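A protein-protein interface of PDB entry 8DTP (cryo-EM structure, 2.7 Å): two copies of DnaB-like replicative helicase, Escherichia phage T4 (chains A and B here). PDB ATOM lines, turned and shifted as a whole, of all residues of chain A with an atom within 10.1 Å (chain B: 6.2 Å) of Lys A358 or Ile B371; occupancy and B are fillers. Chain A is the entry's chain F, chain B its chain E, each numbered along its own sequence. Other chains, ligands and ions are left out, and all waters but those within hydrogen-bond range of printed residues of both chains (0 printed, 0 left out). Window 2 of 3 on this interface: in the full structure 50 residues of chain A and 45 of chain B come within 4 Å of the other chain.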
ATOM      1  N   ALA A 197      13.816  -3.616   8.580  1.00  0.00           N
ATOM      2  CA  ALA A 197      15.158  -4.181   8.611  1.00  0.00           C
ATOM      3  C   ALA A 197      15.449  -4.777   7.243  1.00  0.00           C
ATOM      4  O   ALA A 197      14.552  -4.941   6.412  1.00  0.00           O
ATOM      5  CB  ALA A 197      15.298  -5.232   9.712  1.00  0.00           C
ATOM      6  N   GLY A 198      16.720  -5.097   7.018  1.00  0.00           N
ATOM      7  CA  GLY A 198      17.128  -5.758   5.800  1.00  0.00           C
ATOM      8  C   GLY A 198      16.774  -7.231   5.811  1.00  0.00           C
ATOM      9  O   GLY A 198      16.234  -7.774   6.774  1.00  0.00           O
ATOM     10  N   VAL A 199      17.087  -7.892   4.698  1.00  0.00           N
ATOM     11  CA  VAL A 199      16.800  -9.315   4.577  1.00  0.00           C
ATOM     12  C   VAL A 199      17.770 -10.108   5.441  1.00  0.00           C
ATOM     13  O   VAL A 199      18.989  -9.896   5.389  1.00  0.00           O
ATOM     14  CB  VAL A 199      16.876  -9.761   3.111  1.00  0.00           C
ATOM     15  CG1 VAL A 199      16.946 -11.273   3.034  1.00  0.00           C
ATOM     16  CG2 VAL A 199      15.676  -9.245   2.339  1.00  0.00           C
ATOM     17  N   GLN A 355      10.402  -4.379   4.957  1.00  0.00           N
ATOM     18  CA  GLN A 355      11.736  -4.606   4.421  1.00  0.00           C
ATOM     19  C   GLN A 355      12.268  -3.334   3.772  1.00  0.00           C
ATOM     20  O   GLN A 355      11.554  -2.669   3.016  1.00  0.00           O
ATOM     21  CB  GLN A 355      11.712  -5.751   3.409  1.00  0.00           C
ATOM     22  CG  GLN A 355      13.029  -6.007   2.706  1.00  0.00           C
ATOM     23  CD  GLN A 355      12.947  -7.176   1.744  1.00  0.00           C
ATOM     24  OE1 GLN A 355      12.218  -8.139   1.981  1.00  0.00           O
ATOM     25  NE2 GLN A 355      13.692  -7.095   0.647  1.00  0.00           N
ATOM     26  N   VAL A 356      13.523  -3.005   4.069  1.00  0.00           N
ATOM     27  CA  VAL A 356      14.173  -1.832   3.497  1.00  0.00           C
ATOM     28  C   VAL A 356      14.658  -2.164   2.092  1.00  0.00           C
ATOM     29  O   VAL A 356      14.693  -3.334   1.697  1.00  0.00           O
ATOM     30  CB  VAL A 356      15.334  -1.347   4.383  1.00  0.00           C
ATOM     31  CG1 VAL A 356      14.819  -0.948   5.757  1.00  0.00           C
ATOM     32  CG2 VAL A 356      16.393  -2.428   4.498  1.00  0.00           C
ATOM     33  N   GLY A 357      15.032  -1.138   1.332  1.00  0.00           N
ATOM     34  CA  GLY A 357      15.494  -1.326  -0.024  1.00  0.00           C
ATOM     35  C   GLY A 357      16.883  -1.928  -0.090  1.00  0.00           C
ATOM     36  O   GLY A 357      17.591  -2.066   0.908  1.00  0.00           O
ATOM     37  N   LYS A 358      17.274  -2.296  -1.312  1.00  0.00           N
ATOM     38  CA  LYS A 358      18.575  -2.926  -1.519  1.00  0.00           C
ATOM     39  C   LYS A 358      19.713  -1.982  -1.150  1.00  0.00           C
ATOM     40  O   LYS A 358      20.791  -2.430  -0.745  1.00  0.00           O
ATOM     41  CB  LYS A 358      18.703  -3.388  -2.970  1.00  0.00           C
ATOM     42  CG  LYS A 358      19.917  -4.258  -3.242  1.00  0.00           C
ATOM     43  CD  LYS A 358      19.869  -4.859  -4.638  1.00  0.00           C
ATOM     44  CE  LYS A 358      19.916  -3.784  -5.708  1.00  0.00           C
ATOM     45  NZ  LYS A 358      19.910  -4.372  -7.076  1.00  0.00           N
ATOM     46  N   GLN A 359      19.491  -0.673  -1.283  1.00  0.00           N
ATOM     47  CA  GLN A 359      20.517   0.295  -0.913  1.00  0.00           C
ATOM     48  C   GLN A 359      20.797   0.261   0.584  1.00  0.00           C
ATOM     49  O   GLN A 359      21.951   0.378   1.012  1.00  0.00           O
ATOM     50  CB  GLN A 359      20.092   1.697  -1.344  1.00  0.00           C
ATOM     51  CG  GLN A 359      19.544   1.771  -2.757  1.00  0.00           C
ATOM     52  CD  GLN A 359      19.118   3.173  -3.144  1.00  0.00           C
ATOM     53  OE1 GLN A 359      19.715   4.158  -2.710  1.00  0.00           O
ATOM     54  NE2 GLN A 359      18.075   3.270  -3.960  1.00  0.00           N
ATOM     55  N   ALA A 360      19.750   0.102   1.397  1.00  0.00           N
ATOM     56  CA  ALA A 360      19.925   0.142   2.845  1.00  0.00           C
ATOM     57  C   ALA A 360      20.624  -1.109   3.360  1.00  0.00           C
ATOM     58  O   ALA A 360      21.139  -1.122   4.484  1.00  0.00           O
ATOM     59  CB  ALA A 360      18.571   0.322   3.530  1.00  0.00           C
ATOM     60  N   TRP A 361      20.638  -2.176   2.563  1.00  0.00           N
ATOM     61  CA  TRP A 361      21.332  -3.395   2.958  1.00  0.00           C
ATOM     62  C   TRP A 361      22.825  -3.131   3.095  1.00  0.00           C
ATOM     63  O   TRP A 361      23.446  -2.540   2.207  1.00  0.00           O
ATOM     64  CB  TRP A 361      21.086  -4.504   1.934  1.00  0.00           C
ATOM     65  CG  TRP A 361      19.648  -4.877   1.770  1.00  0.00           C
ATOM     66  CD1 TRP A 361      18.595  -4.429   2.508  1.00  0.00           C
ATOM     67  CD2 TRP A 361      19.102  -5.776   0.799  1.00  0.00           C
ATOM     68  NE1 TRP A 361      17.427  -4.992   2.058  1.00  0.00           N
ATOM     69  CE2 TRP A 361      17.712  -5.825   1.009  1.00  0.00           C
ATOM     70  CE3 TRP A 361      19.655  -6.547  -0.227  1.00  0.00           C
ATOM     71  CZ2 TRP A 361      16.866  -6.610   0.233  1.00  0.00           C
ATOM     72  CZ3 TRP A 361      18.814  -7.327  -0.997  1.00  0.00           C
ATOM     73  CH2 TRP A 361      17.435  -7.352  -0.763  1.00  0.00           C
ATOM     74  N   ASP A 362      23.393  -3.571   4.218  1.00  0.00           N
ATOM     75  CA  ASP A 362      24.814  -3.383   4.517  1.00  0.00           C
ATOM     76  C   ASP A 362      25.202  -1.905   4.475  1.00  0.00           C
ATOM     77  O   ASP A 362      26.295  -1.543   4.035  1.00  0.00           O
ATOM     78  CB  ASP A 362      25.692  -4.205   3.570  1.00  0.00           C
ATOM     79  CG  ASP A 362      25.446  -5.696   3.696  1.00  0.00           C
ATOM     80  OD1 ASP A 362      25.081  -6.148   4.803  1.00  0.00           O
ATOM     81  OD2 ASP A 362      25.618  -6.416   2.691  1.00  0.00           O
ATOM     82  N   SER A 363      24.299  -1.046   4.937  1.00  0.00           N
ATOM     83  CA  SER A 363      24.540   0.389   5.024  1.00  0.00           C
ATOM     84  C   SER A 363      24.541   0.805   6.488  1.00  0.00           C
ATOM     85  O   SER A 363      23.581   0.532   7.214  1.00  0.00           O
ATOM     86  CB  SER A 363      23.481   1.174   4.249  1.00  0.00           C
ATOM     87  OG  SER A 363      23.714   2.568   4.339  1.00  0.00           O
ATOM     88  N   SER A 364      25.612   1.482   6.911  1.00  0.00           N
ATOM     89  CA  SER A 364      25.776   1.832   8.317  1.00  0.00           C
ATOM     90  C   SER A 364      24.725   2.819   8.808  1.00  0.00           C
ATOM     91  O   SER A 364      24.583   2.996  10.022  1.00  0.00           O
ATOM     92  CB  SER A 364      27.175   2.403   8.556  1.00  0.00           C
ATOM     93  OG  SER A 364      27.385   3.577   7.791  1.00  0.00           O
ATOM     94  N   ASP A 365      23.997   3.470   7.904  1.00  0.00           N
ATOM     95  CA  ASP A 365      22.939   4.394   8.284  1.00  0.00           C
ATOM     96  C   ASP A 365      21.804   4.296   7.277  1.00  0.00           C
ATOM     97  O   ASP A 365      22.042   4.126   6.078  1.00  0.00           O
ATOM     98  CB  ASP A 365      23.454   5.838   8.358  1.00  0.00           C
ATOM     99  CG  ASP A 365      22.440   6.790   8.966  1.00  0.00           C
ATOM    100  OD1 ASP A 365      21.411   6.315   9.489  1.00  0.00           O
ATOM    101  OD2 ASP A 365      22.673   8.016   8.918  1.00  0.00           O
ATOM    102  N   VAL A 366      20.571   4.403   7.772  1.00  0.00           N
ATOM    103  CA  VAL A 366      19.381   4.362   6.934  1.00  0.00           C
ATOM    104  C   VAL A 366      18.508   5.563   7.271  1.00  0.00           C
ATOM    105  O   VAL A 366      18.645   6.189   8.323  1.00  0.00           O
ATOM    106  CB  VAL A 366      18.578   3.053   7.101  1.00  0.00           C
ATOM    107  CG1 VAL A 366      19.483   1.838   6.963  1.00  0.00           C
ATOM    108  CG2 VAL A 366      17.843   3.044   8.432  1.00  0.00           C
ATOM    109  N   SER A 369      14.248   7.466   3.078  1.00  0.00           N
ATOM    110  CA  SER A 369      14.431   7.152   1.661  1.00  0.00           C
ATOM    111  C   SER A 369      15.203   5.849   1.484  1.00  0.00           C
ATOM    112  O   SER A 369      16.189   5.767   0.755  1.00  0.00           O
ATOM    113  CB  SER A 369      15.131   8.306   0.957  1.00  0.00           C
ATOM    114  OG  SER A 369      15.289   8.039  -0.425  1.00  0.00           O
ATOM    115  N   ASP A 370      14.736   4.810   2.178  1.00  0.00           N
ATOM    116  CA  ASP A 370      15.288   3.469   2.058  1.00  0.00           C
ATOM    117  C   ASP A 370      14.224   2.385   2.071  1.00  0.00           C
ATOM    118  O   ASP A 370      14.557   1.219   1.830  1.00  0.00           O
ATOM    119  CB  ASP A 370      16.293   3.191   3.189  1.00  0.00           C
ATOM    120  CG  ASP A 370      17.523   4.074   3.107  1.00  0.00           C
ATOM    121  OD1 ASP A 370      17.435   5.257   3.493  1.00  0.00           O
ATOM    122  OD2 ASP A 370      18.579   3.584   2.656  1.00  0.00           O
ATOM    123  N   ILE A 371      12.966   2.725   2.350  1.00  0.00           N
ATOM    124  CA  ILE A 371      11.899   1.734   2.370  1.00  0.00           C
ATOM    125  C   ILE A 371      11.674   1.209   0.961  1.00  0.00           C
ATOM    126  O   ILE A 371      11.566   1.982   0.001  1.00  0.00           O
ATOM    127  CB  ILE A 371      10.615   2.343   2.947  1.00  0.00           C
ATOM    128  CG1 ILE A 371      10.955   3.239   4.135  1.00  0.00           C
ATOM    129  CG2 ILE A 371       9.648   1.244   3.355  1.00  0.00           C
ATOM    130  CD1 ILE A 371       9.964   4.342   4.352  1.00  0.00           C
ATOM    131  N   ALA A 372      11.597  -0.114   0.831  1.00  0.00           N
ATOM    132  CA  ALA A 372      11.533  -0.723  -0.490  1.00  0.00           C
ATOM    133  C   ALA A 372      10.143  -0.597  -1.100  1.00  0.00           C
ATOM    134  O   ALA A 372       9.966   0.028  -2.152  1.00  0.00           O
ATOM    135  CB  ALA A 372      11.950  -2.194  -0.406  1.00  0.00           C
ATOM    136  N   GLU A 373       9.139  -1.178  -0.445  1.00  0.00           N
ATOM    137  CA  GLU A 373       7.835  -1.334  -1.079  1.00  0.00           C
ATOM    138  C   GLU A 373       7.089  -0.008  -1.177  1.00  0.00           C
ATOM    139  O   GLU A 373       6.530   0.321  -2.230  1.00  0.00           O
ATOM    140  CB  GLU A 373       7.014  -2.366  -0.312  1.00  0.00           C
ATOM    141  CG  GLU A 373       7.612  -3.762  -0.336  1.00  0.00           C
ATOM    142  CD  GLU A 373       6.920  -4.706   0.622  1.00  0.00           C
ATOM    143  OE1 GLU A 373       6.183  -4.217   1.503  1.00  0.00           O
ATOM    144  OE2 GLU A 373       7.114  -5.933   0.495  1.00  0.00           O
ATOM    145  N   THR A 390      25.064  -4.396  10.053  1.00  0.00           N
ATOM    146  CA  THR A 390      25.587  -4.538   8.699  1.00  0.00           C
ATOM    147  C   THR A 390      26.855  -5.380   8.602  1.00  0.00           C
ATOM    148  O   THR A 390      26.836  -6.461   8.004  1.00  0.00           O
ATOM    149  CB  THR A 390      25.854  -3.155   8.104  1.00  0.00           C
ATOM    150  OG1 THR A 390      26.850  -2.483   8.885  1.00  0.00           O
ATOM    151  CG2 THR A 390      24.581  -2.332   8.107  1.00  0.00           C
ATOM    152  N   MET B 196      24.676 -18.268  -6.192  1.00  0.00           N
ATOM    153  CA  MET B 196      24.925 -17.105  -7.029  1.00  0.00           C
ATOM    154  C   MET B 196      26.416 -16.810  -7.117  1.00  0.00           C
ATOM    155  O   MET B 196      27.180 -17.083  -6.186  1.00  0.00           O
ATOM    156  CB  MET B 196      24.181 -15.874  -6.500  1.00  0.00           C
ATOM    157  CG  MET B 196      24.798 -15.232  -5.271  1.00  0.00           C
ATOM    158  SD  MET B 196      23.934 -13.721  -4.802  1.00  0.00           S
ATOM    159  CE  MET B 196      25.149 -12.947  -3.740  1.00  0.00           C
ATOM    160  N   TYR B 312      19.121 -21.743 -14.411  1.00  0.00           N
ATOM    161  CA  TYR B 312      19.116 -20.331 -13.949  1.00  0.00           C
ATOM    162  C   TYR B 312      17.669 -19.840 -13.849  1.00  0.00           C
ATOM    163  O   TYR B 312      16.888 -20.110 -14.779  1.00  0.00           O
ATOM    164  CB  TYR B 312      19.974 -19.465 -14.876  1.00  0.00           C
ATOM    165  CG  TYR B 312      20.106 -18.022 -14.458  1.00  0.00           C
ATOM    166  CD1 TYR B 312      19.685 -17.600 -13.208  1.00  0.00           C
ATOM    167  CD2 TYR B 312      20.673 -17.080 -15.299  1.00  0.00           C
ATOM    168  CE1 TYR B 312      19.800 -16.279 -12.811  1.00  0.00           C
ATOM    169  CE2 TYR B 312      20.792 -15.753 -14.920  1.00  0.00           C
ATOM    170  CZ  TYR B 312      20.357 -15.351 -13.670  1.00  0.00           C
ATOM    171  OH  TYR B 312      20.472 -14.049 -13.277  1.00  0.00           O
ATOM    172  N   ALA B 354      21.982 -17.658  -9.668  1.00  0.00           N
ATOM    173  CA  ALA B 354      21.639 -16.254  -9.818  1.00  0.00           C
ATOM    174  C   ALA B 354      22.862 -15.495 -10.305  1.00  0.00           C
ATOM    175  O   ALA B 354      23.999 -15.845  -9.979  1.00  0.00           O
ATOM    176  CB  ALA B 354      21.129 -15.648  -8.505  1.00  0.00           C
ATOM    177  N   GLN B 355      22.618 -14.449 -11.084  1.00  0.00           N
ATOM    178  CA  GLN B 355      23.697 -13.627 -11.603  1.00  0.00           C
ATOM    179  C   GLN B 355      23.976 -12.453 -10.673  1.00  0.00           C
ATOM    180  O   GLN B 355      23.116 -12.006  -9.910  1.00  0.00           O
ATOM    181  CB  GLN B 355      23.367 -13.119 -13.006  1.00  0.00           C
ATOM    182  CG  GLN B 355      23.457 -14.177 -14.095  1.00  0.00           C
ATOM    183  CD  GLN B 355      24.883 -14.540 -14.453  1.00  0.00           C
ATOM    184  OE1 GLN B 355      25.835 -13.940 -13.956  1.00  0.00           O
ATOM    185  NE2 GLN B 355      25.038 -15.528 -15.325  1.00  0.00           N
ATOM    186  N   VAL B 356      25.207 -11.961 -10.745  1.00  0.00           N
ATOM    187  CA  VAL B 356      25.669 -10.832  -9.950  1.00  0.00           C
ATOM    188  C   VAL B 356      25.949  -9.672 -10.892  1.00  0.00           C
ATOM    189  O   VAL B 356      26.500  -9.867 -11.983  1.00  0.00           O
ATOM    190  CB  VAL B 356      26.920 -11.206  -9.132  1.00  0.00           C
ATOM    191  CG1 VAL B 356      27.550  -9.973  -8.507  1.00  0.00           C
ATOM    192  CG2 VAL B 356      26.567 -12.225  -8.062  1.00  0.00           C
ATOM    193  N   GLY B 357      25.553  -8.469 -10.483  1.00  0.00           N
ATOM    194  CA  GLY B 357      25.809  -7.296 -11.294  1.00  0.00           C
ATOM    195  C   GLY B 357      27.292  -7.060 -11.506  1.00  0.00           C
ATOM    196  O   GLY B 357      28.149  -7.616 -10.818  1.00  0.00           O
ATOM    197  N   GLN B 359      29.209  -4.797 -10.764  1.00  0.00           N
ATOM    198  CA  GLN B 359      29.973  -4.145  -9.708  1.00  0.00           C
ATOM    199  C   GLN B 359      30.790  -5.128  -8.878  1.00  0.00           C
ATOM    200  O   GLN B 359      31.783  -4.722  -8.267  1.00  0.00           O
ATOM    201  CB  GLN B 359      29.037  -3.346  -8.797  1.00  0.00           C
ATOM    202  CG  GLN B 359      27.899  -4.148  -8.185  1.00  0.00           C
ATOM    203  CD  GLN B 359      26.698  -4.263  -9.103  1.00  0.00           C
ATOM    204  OE1 GLN B 359      26.791  -4.011 -10.304  1.00  0.00           O
ATOM    205  NE2 GLN B 359      25.558  -4.642  -8.539  1.00  0.00           N
ATOM    206  N   VAL B 366      31.354 -10.473  -2.328  1.00  0.00           N
ATOM    207  CA  VAL B 366      30.063 -10.159  -2.924  1.00  0.00           C
ATOM    208  C   VAL B 366      29.021 -10.133  -1.816  1.00  0.00           C
ATOM    209  O   VAL B 366      29.009 -11.004  -0.940  1.00  0.00           O
ATOM    210  CB  VAL B 366      29.681 -11.169  -4.028  1.00  0.00           C
ATOM    211  CG1 VAL B 366      29.767 -12.595  -3.514  1.00  0.00           C
ATOM    212  CG2 VAL B 366      28.291 -10.876  -4.572  1.00  0.00           C
ATOM    213  N   ASN B 367      28.159  -9.123  -1.842  1.00  0.00           N
ATOM    214  CA  ASN B 367      27.105  -8.960  -0.854  1.00  0.00           C
ATOM    215  C   ASN B 367      25.755  -9.313  -1.463  1.00  0.00           C
ATOM    216  O   ASN B 367      25.631  -9.566  -2.664  1.00  0.00           O
ATOM    217  CB  ASN B 367      27.088  -7.527  -0.307  1.00  0.00           C
ATOM    218  CG  ASN B 367      28.361  -7.172   0.432  1.00  0.00           C
ATOM    219  OD1 ASN B 367      29.334  -6.719  -0.167  1.00  0.00           O
ATOM    220  ND2 ASN B 367      28.359  -7.373   1.744  1.00  0.00           N
ATOM    221  N   MET B 368      24.733  -9.334  -0.605  1.00  0.00           N
ATOM    222  CA  MET B 368      23.381  -9.618  -1.073  1.00  0.00           C
ATOM    223  C   MET B 368      22.874  -8.533  -2.011  1.00  0.00           C
ATOM    224  O   MET B 368      22.065  -8.813  -2.903  1.00  0.00           O
ATOM    225  CB  MET B 368      22.435  -9.773   0.116  1.00  0.00           C
ATOM    226  CG  MET B 368      21.050 -10.271  -0.249  1.00  0.00           C
ATOM    227  SD  MET B 368      19.902 -10.216   1.138  1.00  0.00           S
ATOM    228  CE  MET B 368      20.763 -11.226   2.337  1.00  0.00           C
ATOM    229  N   SER B 369      23.338  -7.293  -1.831  1.00  0.00           N
ATOM    230  CA  SER B 369      22.933  -6.202  -2.709  1.00  0.00           C
ATOM    231  C   SER B 369      23.454  -6.378  -4.129  1.00  0.00           C
ATOM    232  O   SER B 369      22.950  -5.720  -5.045  1.00  0.00           O
ATOM    233  CB  SER B 369      23.413  -4.866  -2.143  1.00  0.00           C
ATOM    234  OG  SER B 369      24.825  -4.834  -2.047  1.00  0.00           O
ATOM    235  N   ASP B 370      24.444  -7.240  -4.331  1.00  0.00           N
ATOM    236  CA  ASP B 370      25.002  -7.492  -5.658  1.00  0.00           C
ATOM    237  C   ASP B 370      24.260  -8.617  -6.373  1.00  0.00           C
ATOM    238  O   ASP B 370      24.854  -9.594  -6.821  1.00  0.00           O
ATOM    239  CB  ASP B 370      26.488  -7.804  -5.542  1.00  0.00           C
ATOM    240  CG  ASP B 370      27.258  -6.711  -4.835  1.00  0.00           C
ATOM    241  OD1 ASP B 370      26.873  -5.530  -4.964  1.00  0.00           O
ATOM    242  OD2 ASP B 370      28.248  -7.031  -4.148  1.00  0.00           O
ATOM    243  N   ILE B 371      22.940  -8.489  -6.478  1.00  0.00           N
ATOM    244  CA  ILE B 371      22.111  -9.426  -7.225  1.00  0.00           C
ATOM    245  C   ILE B 371      21.698  -8.741  -8.521  1.00  0.00           C
ATOM    246  O   ILE B 371      21.087  -7.665  -8.499  1.00  0.00           O
ATOM    247  CB  ILE B 371      20.892  -9.887  -6.407  1.00  0.00           C
ATOM    248  CG1 ILE B 371      19.921 -10.684  -7.282  1.00  0.00           C
ATOM    249  CG2 ILE B 371      20.203  -8.708  -5.726  1.00  0.00           C
ATOM    250  CD1 ILE B 371      20.479 -12.010  -7.754  1.00  0.00           C
ATOM    251  N   ALA B 372      22.058  -9.353  -9.652  1.00  0.00           N
ATOM    252  CA  ALA B 372      21.854  -8.705 -10.944  1.00  0.00           C
ATOM    253  C   ALA B 372      20.375  -8.489 -11.228  1.00  0.00           C
ATOM    254  O   ALA B 372      19.978  -7.436 -11.739  1.00  0.00           O
ATOM    255  CB  ALA B 372      22.499  -9.534 -12.055  1.00  0.00           C
ATOM    256  N   GLU B 373      19.547  -9.470 -10.906  1.00  0.00           N
ATOM    257  CA  GLU B 373      18.114  -9.383 -11.137  1.00  0.00           C
ATOM    258  C   GLU B 373      17.444  -8.804  -9.889  1.00  0.00           C
ATOM    259  O   GLU B 373      18.116  -8.249  -9.016  1.00  0.00           O
ATOM    260  CB  GLU B 373      17.566 -10.756 -11.538  1.00  0.00           C
ATOM    261  CG  GLU B 373      18.076 -11.273 -12.880  1.00  0.00           C
ATOM    262  CD  GLU B 373      17.568 -10.470 -14.066  1.00  0.00           C
ATOM    263  OE1 GLU B 373      16.671  -9.620 -13.887  1.00  0.00           O
ATOM    264  OE2 GLU B 373      18.069 -10.695 -15.186  1.00  0.00           O
ATOM    265  N   SER B 374      16.116  -8.906  -9.817  1.00  0.00           N
ATOM    266  CA  SER B 374      15.340  -8.350  -8.715  1.00  0.00           C
ATOM    267  C   SER B 374      15.919  -8.722  -7.356  1.00  0.00           C
ATOM    268  O   SER B 374      16.459  -9.813  -7.167  1.00  0.00           O
ATOM    269  CB  SER B 374      13.895  -8.844  -8.807  1.00  0.00           C
ATOM    270  OG  SER B 374      13.279  -8.873  -7.533  1.00  0.00           O
ATOM    271  N   ALA B 375      15.784  -7.800  -6.404  1.00  0.00           N
ATOM    272  CA  ALA B 375      16.142  -8.054  -5.015  1.00  0.00           C
ATOM    273  C   ALA B 375      15.059  -8.819  -4.269  1.00  0.00           C
ATOM    274  O   ALA B 375      15.228  -9.101  -3.078  1.00  0.00           O
ATOM    275  CB  ALA B 375      16.435  -6.737  -4.293  1.00  0.00           C
ATOM    276  N   LEU B 377      14.338 -11.859  -5.233  1.00  0.00           N
ATOM    277  CA  LEU B 377      14.916 -13.200  -5.173  1.00  0.00           C
ATOM    278  C   LEU B 377      15.637 -13.452  -3.857  1.00  0.00           C
ATOM    279  O   LEU B 377      15.432 -14.526  -3.265  1.00  0.00           O
ATOM    280  CB  LEU B 377      15.828 -13.429  -6.383  1.00  0.00           C
ATOM    281  CG  LEU B 377      16.574 -14.763  -6.429  1.00  0.00           C
ATOM    282  CD1 LEU B 377      15.603 -15.930  -6.366  1.00  0.00           C
ATOM    283  CD2 LEU B 377      17.440 -14.851  -7.674  1.00  0.00           C
ATOM    284  N   PRO B 378      16.479 -12.537  -3.333  1.00  0.00           N
ATOM    285  CA  PRO B 378      16.948 -12.712  -1.953  1.00  0.00           C
ATOM    286  C   PRO B 378      15.919 -12.268  -0.929  1.00  0.00           C
ATOM    287  O   PRO B 378      16.262 -11.628   0.067  1.00  0.00           O
ATOM    288  CB  PRO B 378      18.200 -11.831  -1.894  1.00  0.00           C
ATOM    289  CG  PRO B 378      17.961 -10.789  -2.896  1.00  0.00           C
ATOM    290  CD  PRO B 378      17.220 -11.460  -4.015  1.00  0.00           C
ATOM    291  N   MET B 384      20.831 -18.797   0.255  1.00  0.00           N
ATOM    292  CA  MET B 384      21.500 -18.179  -0.915  1.00  0.00           C
ATOM    293  C   MET B 384      23.007 -18.113  -0.662  1.00  0.00           C
ATOM    294  O   MET B 384      23.481 -17.087  -0.167  1.00  0.00           O
ATOM    295  CB  MET B 384      20.950 -16.771  -1.163  1.00  0.00           C
ATOM    296  CG  MET B 384      21.781 -15.929  -2.101  1.00  0.00           C
ATOM    297  SD  MET B 384      20.877 -14.433  -2.542  1.00  0.00           S
ATOM    298  CE  MET B 384      19.237 -15.112  -2.778  1.00  0.00           C
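Positions printed for both chains: 355, 356, 357, 359, 366, 369, 370, 371, 372 and 373.
Lys A358 touches just these residues of chain B: Ser B369, Ile B371 and Ala B375. Of the printed residues of chain B, Asp A362 touches Asn B367. No residue of chain A comes within 4 Å of Val B356. Printed residues of chain A within 4 Å of Asn B367: Asp A362. Of chain A, only Lys A358 comes within 4 Å of Ser B369. Ile B371 touches just one residue of chain A: Lys A358 (3.8 Å). Ala B372 touches none of the printed residues of chain A. Glu B373 touches none of the printed residues of chain A. The nearest residue of chain B that does not touch Lys A358 is Glu B373 (4.7 Å).
Among the printed residues, pairs that only touch across the chains: Val A199 with Pro B378, Lys A358 with Ser B369, Val A199 with Met B368, Trp A361 with Ala B375, Trp A361 with Met B368, Lys A358 with Ile B371 and Lys A358 with Ala B375.
The backbone NH of Asn B367 sits at hydrogen-bond distance from the side-chain carboxylate of Asp B370, 3.1 Å away. The indole nitrogen (NE1) of Trp A361 is in hydrogen-bond range of the backbone carbonyl oxygen (O) of Val A356 (3.2 Å). NE1 of Trp A361 sits close to O of Gly A357 (3.1 Å).
Of the 20 printed residues of chain B, 6 touch a printed residue of chain A. Hydrophobic or aromatic side chains of chain B that line the printed part of chain A: Met B368 and Ala B375. Of the 21 printed residues of chain A, 4 touch a printed residue of chain B. Printed residues of chain A that touch a printed residue of chain B: Val A199, Lys A358, Trp A361 and Asp A362.
The side-chain amide nitrogen (ND2) of Asn B367 sits at hydrogen-bond distance from the side-chain carboxylate (OD2) of Asp A362, 3.1 Å away.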
